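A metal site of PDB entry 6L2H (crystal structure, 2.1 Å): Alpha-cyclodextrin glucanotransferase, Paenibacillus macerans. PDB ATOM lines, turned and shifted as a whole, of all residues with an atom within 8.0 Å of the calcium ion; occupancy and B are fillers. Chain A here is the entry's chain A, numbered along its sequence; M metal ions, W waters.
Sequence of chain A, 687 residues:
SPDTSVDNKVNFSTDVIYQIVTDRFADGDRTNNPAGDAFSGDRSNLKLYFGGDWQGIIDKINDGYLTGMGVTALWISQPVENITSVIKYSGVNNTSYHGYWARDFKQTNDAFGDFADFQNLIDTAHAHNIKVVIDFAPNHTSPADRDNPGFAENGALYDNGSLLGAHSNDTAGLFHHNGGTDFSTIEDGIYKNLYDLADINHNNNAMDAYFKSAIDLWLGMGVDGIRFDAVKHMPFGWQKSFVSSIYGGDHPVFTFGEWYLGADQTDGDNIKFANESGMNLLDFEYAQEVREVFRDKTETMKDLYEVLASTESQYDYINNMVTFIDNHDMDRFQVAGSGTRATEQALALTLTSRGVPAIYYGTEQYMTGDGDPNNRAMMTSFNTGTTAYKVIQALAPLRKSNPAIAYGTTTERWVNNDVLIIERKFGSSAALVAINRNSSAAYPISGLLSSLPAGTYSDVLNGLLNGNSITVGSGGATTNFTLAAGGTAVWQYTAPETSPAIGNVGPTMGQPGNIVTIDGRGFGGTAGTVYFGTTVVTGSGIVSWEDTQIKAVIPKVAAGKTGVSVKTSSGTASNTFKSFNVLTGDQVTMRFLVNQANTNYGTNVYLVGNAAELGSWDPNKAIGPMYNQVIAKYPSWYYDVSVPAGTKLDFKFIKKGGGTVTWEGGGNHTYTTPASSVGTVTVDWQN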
ATOM      1  N   THR A  22     -30.306  14.120 -31.637  1.00  0.00           N
ATOM      2  CA  THR A  22     -29.524  13.698 -30.476  1.00  0.00           C
ATOM      3  C   THR A  22     -28.291  12.858 -30.816  1.00  0.00           C
ATOM      4  O   THR A  22     -27.223  13.065 -30.223  1.00  0.00           O
ATOM      5  CB  THR A  22     -30.408  12.925 -29.495  1.00  0.00           C
ATOM      6  OG1 THR A  22     -31.521  13.759 -29.118  1.00  0.00           O
ATOM      7  CG2 THR A  22     -29.633  12.557 -28.239  1.00  0.00           C
ATOM      8  N   ASP A  23     -28.416  11.945 -31.763  1.00  0.00           N
ATOM      9  CA  ASP A  23     -27.324  11.036 -32.104  1.00  0.00           C
ATOM     10  C   ASP A  23     -26.185  11.770 -32.789  1.00  0.00           C
ATOM     11  O   ASP A  23     -25.051  11.280 -32.832  1.00  0.00           O
ATOM     12  CB  ASP A  23     -27.831   9.906 -33.006  1.00  0.00           C
ATOM     13  CG  ASP A  23     -26.732   8.899 -33.356  1.00  0.00           C
ATOM     14  OD1 ASP A  23     -26.271   8.182 -32.449  1.00  0.00           O
ATOM     15  OD2 ASP A  23     -26.345   8.819 -34.546  1.00  0.00           O
ATOM     16  N   ALA A  26     -23.500  15.327 -29.632  1.00  0.00           N
ATOM     17  CA  ALA A  26     -22.287  15.011 -28.876  1.00  0.00           C
ATOM     18  C   ALA A  26     -22.372  13.678 -28.127  1.00  0.00           C
ATOM     19  O   ALA A  26     -23.315  13.439 -27.368  1.00  0.00           O
ATOM     20  CB  ALA A  26     -21.981  16.130 -27.883  1.00  0.00           C
ATOM     21  N   ASP A  27     -21.377  12.819 -28.327  1.00  0.00           N
ATOM     22  CA  ASP A  27     -21.278  11.530 -27.630  1.00  0.00           C
ATOM     23  C   ASP A  27     -20.653  11.740 -26.262  1.00  0.00           C
ATOM     24  O   ASP A  27     -19.444  11.655 -26.117  1.00  0.00           O
ATOM     25  CB  ASP A  27     -20.455  10.530 -28.449  1.00  0.00           C
ATOM     26  CG  ASP A  27     -20.395   9.138 -27.822  1.00  0.00           C
ATOM     27  OD1 ASP A  27     -21.060   8.875 -26.793  1.00  0.00           O
ATOM     28  OD2 ASP A  27     -19.683   8.287 -28.397  1.00  0.00           O
ATOM     29  N   GLY A  28     -21.476  12.006 -25.257  1.00  0.00           N
ATOM     30  CA  GLY A  28     -20.979  12.275 -23.921  1.00  0.00           C
ATOM     31  C   GLY A  28     -20.746  11.037 -23.090  1.00  0.00           C
ATOM     32  O   GLY A  28     -20.165  11.107 -22.014  1.00  0.00           O
ATOM     33  N   ASP A  29     -21.221   9.897 -23.580  1.00  0.00           N
ATOM     34  CA  ASP A  29     -21.104   8.627 -22.863  1.00  0.00           C
ATOM     35  C   ASP A  29     -20.932   7.517 -23.887  1.00  0.00           C
ATOM     36  O   ASP A  29     -21.885   7.089 -24.504  1.00  0.00           O
ATOM     37  CB  ASP A  29     -22.333   8.379 -21.983  1.00  0.00           C
ATOM     38  CG  ASP A  29     -22.218   7.127 -21.125  1.00  0.00           C
ATOM     39  OD1 ASP A  29     -21.177   6.443 -21.206  1.00  0.00           O
ATOM     40  OD2 ASP A  29     -23.167   6.809 -20.378  1.00  0.00           O
ATOM     41  N   ARG A  30     -19.704   7.056 -24.056  1.00  0.00           N
ATOM     42  CA  ARG A  30     -19.436   6.019 -25.054  1.00  0.00           C
ATOM     43  C   ARG A  30     -19.948   4.653 -24.601  1.00  0.00           C
ATOM     44  O   ARG A  30     -20.100   3.751 -25.417  1.00  0.00           O
ATOM     45  CB  ARG A  30     -17.937   5.970 -25.348  1.00  0.00           C
ATOM     46  CG  ARG A  30     -17.440   7.259 -26.014  1.00  0.00           C
ATOM     47  CD  ARG A  30     -15.933   7.314 -26.171  1.00  0.00           C
ATOM     48  NE  ARG A  30     -15.419   6.239 -27.017  1.00  0.00           N
ATOM     49  CZ  ARG A  30     -14.168   6.183 -27.467  1.00  0.00           C
ATOM     50  NH1 ARG A  30     -13.783   5.166 -28.231  1.00  0.00           N
ATOM     51  NH2 ARG A  30     -13.306   7.150 -27.164  1.00  0.00           N
ATOM     52  N   THR A  31     -20.251   4.520 -23.313  1.00  0.00           N
ATOM     53  CA  THR A  31     -20.677   3.226 -22.773  1.00  0.00           C
ATOM     54  C   THR A  31     -22.107   2.854 -23.179  1.00  0.00           C
ATOM     55  O   THR A  31     -22.490   1.693 -23.059  1.00  0.00           O
ATOM     56  CB  THR A  31     -20.590   3.214 -21.233  1.00  0.00           C
ATOM     57  OG1 THR A  31     -21.573   4.104 -20.675  1.00  0.00           O
ATOM     58  CG2 THR A  31     -19.197   3.629 -20.784  1.00  0.00           C
ATOM     59  N   ASN A  32     -22.887   3.816 -23.656  1.00  0.00           N
ATOM     60  CA  ASN A  32     -24.230   3.497 -24.149  1.00  0.00           C
ATOM     61  C   ASN A  32     -24.280   3.424 -25.669  1.00  0.00           C
ATOM     62  O   ASN A  32     -25.354   3.347 -26.254  1.00  0.00           O
ATOM     63  CB  ASN A  32     -25.246   4.519 -23.631  1.00  0.00           C
ATOM     64  CG  ASN A  32     -24.929   5.955 -24.039  1.00  0.00           C
ATOM     65  OD1 ASN A  32     -24.337   6.202 -25.092  1.00  0.00           O
ATOM     66  ND2 ASN A  32     -25.348   6.915 -23.217  1.00  0.00           N
ATOM     67  N   ASN A  33     -23.118   3.451 -26.312  1.00  0.00           N
ATOM     68  CA  ASN A  33     -23.071   3.357 -27.769  1.00  0.00           C
ATOM     69  C   ASN A  33     -23.510   1.994 -28.264  1.00  0.00           C
ATOM     70  O   ASN A  33     -23.100   0.973 -27.719  1.00  0.00           O
ATOM     71  CB  ASN A  33     -21.658   3.646 -28.289  1.00  0.00           C
ATOM     72  CG  ASN A  33     -21.289   5.103 -28.168  1.00  0.00           C
ATOM     73  OD1 ASN A  33     -22.053   5.908 -27.647  1.00  0.00           O
ATOM     74  ND2 ASN A  33     -20.089   5.452 -28.634  1.00  0.00           N
ATOM     75  N   PRO A  34     -24.360   1.966 -29.292  1.00  0.00           N
ATOM     76  CA  PRO A  34     -24.656   0.698 -29.957  1.00  0.00           C
ATOM     77  C   PRO A  34     -23.392   0.157 -30.607  1.00  0.00           C
ATOM     78  O   PRO A  34     -22.418   0.905 -30.749  1.00  0.00           O
ATOM     79  CB  PRO A  34     -25.708   1.088 -31.006  1.00  0.00           C
ATOM     80  CG  PRO A  34     -26.332   2.348 -30.476  1.00  0.00           C
ATOM     81  CD  PRO A  34     -25.190   3.074 -29.796  1.00  0.00           C
ATOM     82  N   PHE A  39     -23.625   0.539 -35.521  1.00  0.00           N
ATOM     83  CA  PHE A  39     -22.791   1.674 -35.127  1.00  0.00           C
ATOM     84  C   PHE A  39     -21.775   2.047 -36.193  1.00  0.00           C
ATOM     85  O   PHE A  39     -21.154   1.171 -36.781  1.00  0.00           O
ATOM     86  CB  PHE A  39     -22.078   1.353 -33.810  1.00  0.00           C
ATOM     87  CG  PHE A  39     -21.278   2.491 -33.245  1.00  0.00           C
ATOM     88  CD1 PHE A  39     -21.918   3.534 -32.601  1.00  0.00           C
ATOM     89  CD2 PHE A  39     -19.901   2.507 -33.349  1.00  0.00           C
ATOM     90  CE1 PHE A  39     -21.186   4.589 -32.070  1.00  0.00           C
ATOM     91  CE2 PHE A  39     -19.167   3.553 -32.815  1.00  0.00           C
ATOM     92  CZ  PHE A  39     -19.811   4.592 -32.180  1.00  0.00           C
ATOM     93  N   TYR A  49     -26.090   4.560 -36.000  1.00  0.00           N
ATOM     94  CA  TYR A  49     -25.865   5.371 -34.799  1.00  0.00           C
ATOM     95  C   TYR A  49     -24.437   5.900 -34.761  1.00  0.00           C
ATOM     96  O   TYR A  49     -23.475   5.141 -34.942  1.00  0.00           O
ATOM     97  CB  TYR A  49     -26.115   4.544 -33.531  1.00  0.00           C
ATOM     98  CG  TYR A  49     -27.560   4.431 -33.079  1.00  0.00           C
ATOM     99  CD1 TYR A  49     -28.053   5.255 -32.074  1.00  0.00           C
ATOM    100  CD2 TYR A  49     -28.407   3.481 -33.609  1.00  0.00           C
ATOM    101  CE1 TYR A  49     -29.366   5.149 -31.640  1.00  0.00           C
ATOM    102  CE2 TYR A  49     -29.721   3.353 -33.178  1.00  0.00           C
ATOM    103  CZ  TYR A  49     -30.198   4.195 -32.186  1.00  0.00           C
ATOM    104  OH  TYR A  49     -31.487   4.083 -31.747  1.00  0.00           O
ATOM    105  N   PHE A  50     -24.281   7.209 -34.515  1.00  0.00           N
ATOM    106  CA  PHE A  50     -22.959   7.801 -34.360  1.00  0.00           C
ATOM    107  C   PHE A  50     -22.564   7.841 -32.885  1.00  0.00           C
ATOM    108  O   PHE A  50     -21.370   7.874 -32.554  1.00  0.00           O
ATOM    109  CB  PHE A  50     -22.909   9.209 -34.976  1.00  0.00           C
ATOM    110  CG  PHE A  50     -22.760   9.226 -36.481  1.00  0.00           C
ATOM    111  CD1 PHE A  50     -22.881   8.055 -37.225  1.00  0.00           C
ATOM    112  CD2 PHE A  50     -22.475  10.410 -37.141  1.00  0.00           C
ATOM    113  CE1 PHE A  50     -22.739   8.074 -38.602  1.00  0.00           C
ATOM    114  CE2 PHE A  50     -22.324  10.429 -38.522  1.00  0.00           C
ATOM    115  CZ  PHE A  50     -22.462   9.271 -39.254  1.00  0.00           C
ATOM    116  N   GLY A  51     -23.547   7.861 -31.986  1.00  0.00           N
ATOM    117  CA  GLY A  51     -23.272   7.815 -30.570  1.00  0.00           C
ATOM    118  C   GLY A  51     -23.651   9.037 -29.741  1.00  0.00           C
ATOM    119  O   GLY A  51     -23.437   9.050 -28.530  1.00  0.00           O
ATOM    120  N   GLY A  52     -24.199  10.065 -30.374  1.00  0.00           N
ATOM    121  CA  GLY A  52     -24.640  11.252 -29.656  1.00  0.00           C
ATOM    122  C   GLY A  52     -25.743  10.931 -28.658  1.00  0.00           C
ATOM    123  O   GLY A  52     -26.660  10.176 -28.978  1.00  0.00           O
ATOM    124  N   ASP A  53     -25.671  11.511 -27.459  1.00  0.00           N
ATOM    125  CA  ASP A  53     -26.563  11.107 -26.370  1.00  0.00           C
ATOM    126  C   ASP A  53     -26.918  12.280 -25.473  1.00  0.00           C
ATOM    127  O   ASP A  53     -26.506  13.411 -25.717  1.00  0.00           O
ATOM    128  CB  ASP A  53     -25.919   9.993 -25.556  1.00  0.00           C
ATOM    129  CG  ASP A  53     -24.484  10.307 -25.163  1.00  0.00           C
ATOM    130  OD1 ASP A  53     -24.176  11.499 -24.961  1.00  0.00           O
ATOM    131  OD2 ASP A  53     -23.663   9.372 -25.075  1.00  0.00           O
ATOM    132  N   TRP A  54     -27.676  12.010 -24.406  1.00  0.00           N
ATOM    133  CA  TRP A  54     -28.151  13.086 -23.541  1.00  0.00           C
ATOM    134  C   TRP A  54     -27.018  13.665 -22.698  1.00  0.00           C
ATOM    135  O   TRP A  54     -26.998  14.856 -22.412  1.00  0.00           O
ATOM    136  CB  TRP A  54     -29.293  12.587 -22.641  1.00  0.00           C
ATOM    137  CG  TRP A  54     -30.541  12.270 -23.431  1.00  0.00           C
ATOM    138  CD1 TRP A  54     -30.948  12.861 -24.592  1.00  0.00           C
ATOM    139  CD2 TRP A  54     -31.506  11.258 -23.133  1.00  0.00           C
ATOM    140  NE1 TRP A  54     -32.122  12.296 -25.017  1.00  0.00           N
ATOM    141  CE2 TRP A  54     -32.486  11.308 -24.143  1.00  0.00           C
ATOM    142  CE3 TRP A  54     -31.640  10.309 -22.097  1.00  0.00           C
ATOM    143  CZ2 TRP A  54     -33.583  10.447 -24.162  1.00  0.00           C
ATOM    144  CZ3 TRP A  54     -32.738   9.458 -22.119  1.00  0.00           C
ATOM    145  CH2 TRP A  54     -33.699   9.538 -23.137  1.00  0.00           C
ATOM    146  N   GLN A  55     -26.080  12.822 -22.292  1.00  0.00           N
ATOM    147  CA  GLN A  55     -24.910  13.296 -21.580  1.00  0.00           C
ATOM    148  C   GLN A  55     -24.161  14.338 -22.390  1.00  0.00           C
ATOM    149  O   GLN A  55     -23.650  15.319 -21.851  1.00  0.00           O
ATOM    150  CB  GLN A  55     -23.962  12.140 -21.248  1.00  0.00           C
ATOM    151  CG  GLN A  55     -22.798  12.575 -20.371  1.00  0.00           C
ATOM    152  CD  GLN A  55     -23.260  13.085 -19.027  1.00  0.00           C
ATOM    153  OE1 GLN A  55     -23.954  12.376 -18.289  1.00  0.00           O
ATOM    154  NE2 GLN A  55     -22.891  14.310 -18.690  1.00  0.00           N
ATOM    155  N   GLY A  56     -24.085  14.107 -23.702  1.00  0.00           N
ATOM    156  CA  GLY A  56     -23.431  15.036 -24.591  1.00  0.00           C
ATOM    157  C   GLY A  56     -24.126  16.380 -24.557  1.00  0.00           C
ATOM    158  O   GLY A  56     -23.470  17.418 -24.445  1.00  0.00           O
ATOM    159  N   ASP A 110     -31.913   3.521 -24.907  1.00  0.00           N
ATOM    160  CA  ASP A 110     -30.742   3.399 -24.041  1.00  0.00           C
ATOM    161  C   ASP A 110     -29.482   3.930 -24.702  1.00  0.00           C
ATOM    162  O   ASP A 110     -28.500   4.220 -24.030  1.00  0.00           O
ATOM    163  CB  ASP A 110     -30.542   1.951 -23.614  1.00  0.00           C
ATOM    164  CG  ASP A 110     -31.752   1.380 -22.899  1.00  0.00           C
ATOM    165  OD1 ASP A 110     -32.726   2.125 -22.662  1.00  0.00           O
ATOM    166  OD2 ASP A 110     -31.741   0.176 -22.566  1.00  0.00           O
ATOM    167  N   ALA A 111     -29.511   4.066 -26.028  1.00  0.00           N
ATOM    168  CA  ALA A 111     -28.425   4.742 -26.739  1.00  0.00           C
ATOM    169  C   ALA A 111     -28.330   6.212 -26.318  1.00  0.00           C
ATOM    170  O   ALA A 111     -27.238   6.773 -26.270  1.00  0.00           O
ATOM    171  CB  ALA A 111     -28.630   4.636 -28.246  1.00  0.00           C
ATOM    172  N   PHE A 112     -29.464   6.826 -26.016  1.00  0.00           N
ATOM    173  CA  PHE A 112     -29.460   8.227 -25.580  1.00  0.00           C
ATOM    174  C   PHE A 112     -29.163   8.339 -24.086  1.00  0.00           C
ATOM    175  O   PHE A 112     -28.520   9.287 -23.651  1.00  0.00           O
ATOM    176  CB  PHE A 112     -30.804   8.899 -25.894  1.00  0.00           C
ATOM    177  CG  PHE A 112     -31.120   8.975 -27.364  1.00  0.00           C
ATOM    178  CD1 PHE A 112     -30.114   8.864 -28.315  1.00  0.00           C
ATOM    179  CD2 PHE A 112     -32.428   9.142 -27.788  1.00  0.00           C
ATOM    180  CE1 PHE A 112     -30.408   8.932 -29.664  1.00  0.00           C
ATOM    181  CE2 PHE A 112     -32.731   9.210 -29.134  1.00  0.00           C
ATOM    182  CZ  PHE A 112     -31.724   9.112 -30.080  1.00  0.00           C
ATOM    183  N   GLY A 113     -29.637   7.366 -23.314  1.00  0.00           N
ATOM    184  CA  GLY A 113     -29.398   7.312 -21.881  1.00  0.00           C
ATOM    185  C   GLY A 113     -30.494   6.541 -21.164  1.00  0.00           C
ATOM    186  O   GLY A 113     -31.407   6.033 -21.810  1.00  0.00           O
HETATM  187 CA    CA M   1     -23.128   7.613 -26.535  1.00  0.00          CA
HETATM  188  O   HOH W   1     -25.170   6.561 -27.834  1.00  0.00           O
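The side-chain carboxylate of Asp 29 sits at hydrogen-bond distance from the side-chain hydroxyl of Thr 31 (2.4 Å).
The side-chain carboxylate of Asp 53 is in hydrogen-bond range of the backbone NH of Gly 56 (2.9 Å).
O of Ala 26 sits at hydrogen-bond distance from N of Asp 53 (3.0 Å).
N of Gly 51 is in hydrogen-bond range of OD1 of Asp 23 (2.8 Å).
The side-chain carboxylate (OD1) of Asp 53 lies within hydrogen-bond range of the backbone NH (N) of Gly 28 (2.8 Å).
OD1 of Asn 32 lies close to O of Ala 111, at 3.2 Å.
The side-chain amide oxygen (OD1) of Asn 33 is bound to the calcium ion (2.3 Å).
The calcium ion is bound by OD2 of Asp 53 (2.3 Å).
OD1 of Asn 32 is bound to the calcium ion, at 2.4 Å.
OD1 of Asp 27 is bound to the calcium ion, at 2.4 Å.
The backbone carbonyl oxygen (O) of Asp 29 binds the calcium ion (2.4 Å).
O of Gly 51 is bound to the calcium ion (2.5 Å).
Water W1 is bound to the calcium ion (2.6 Å).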
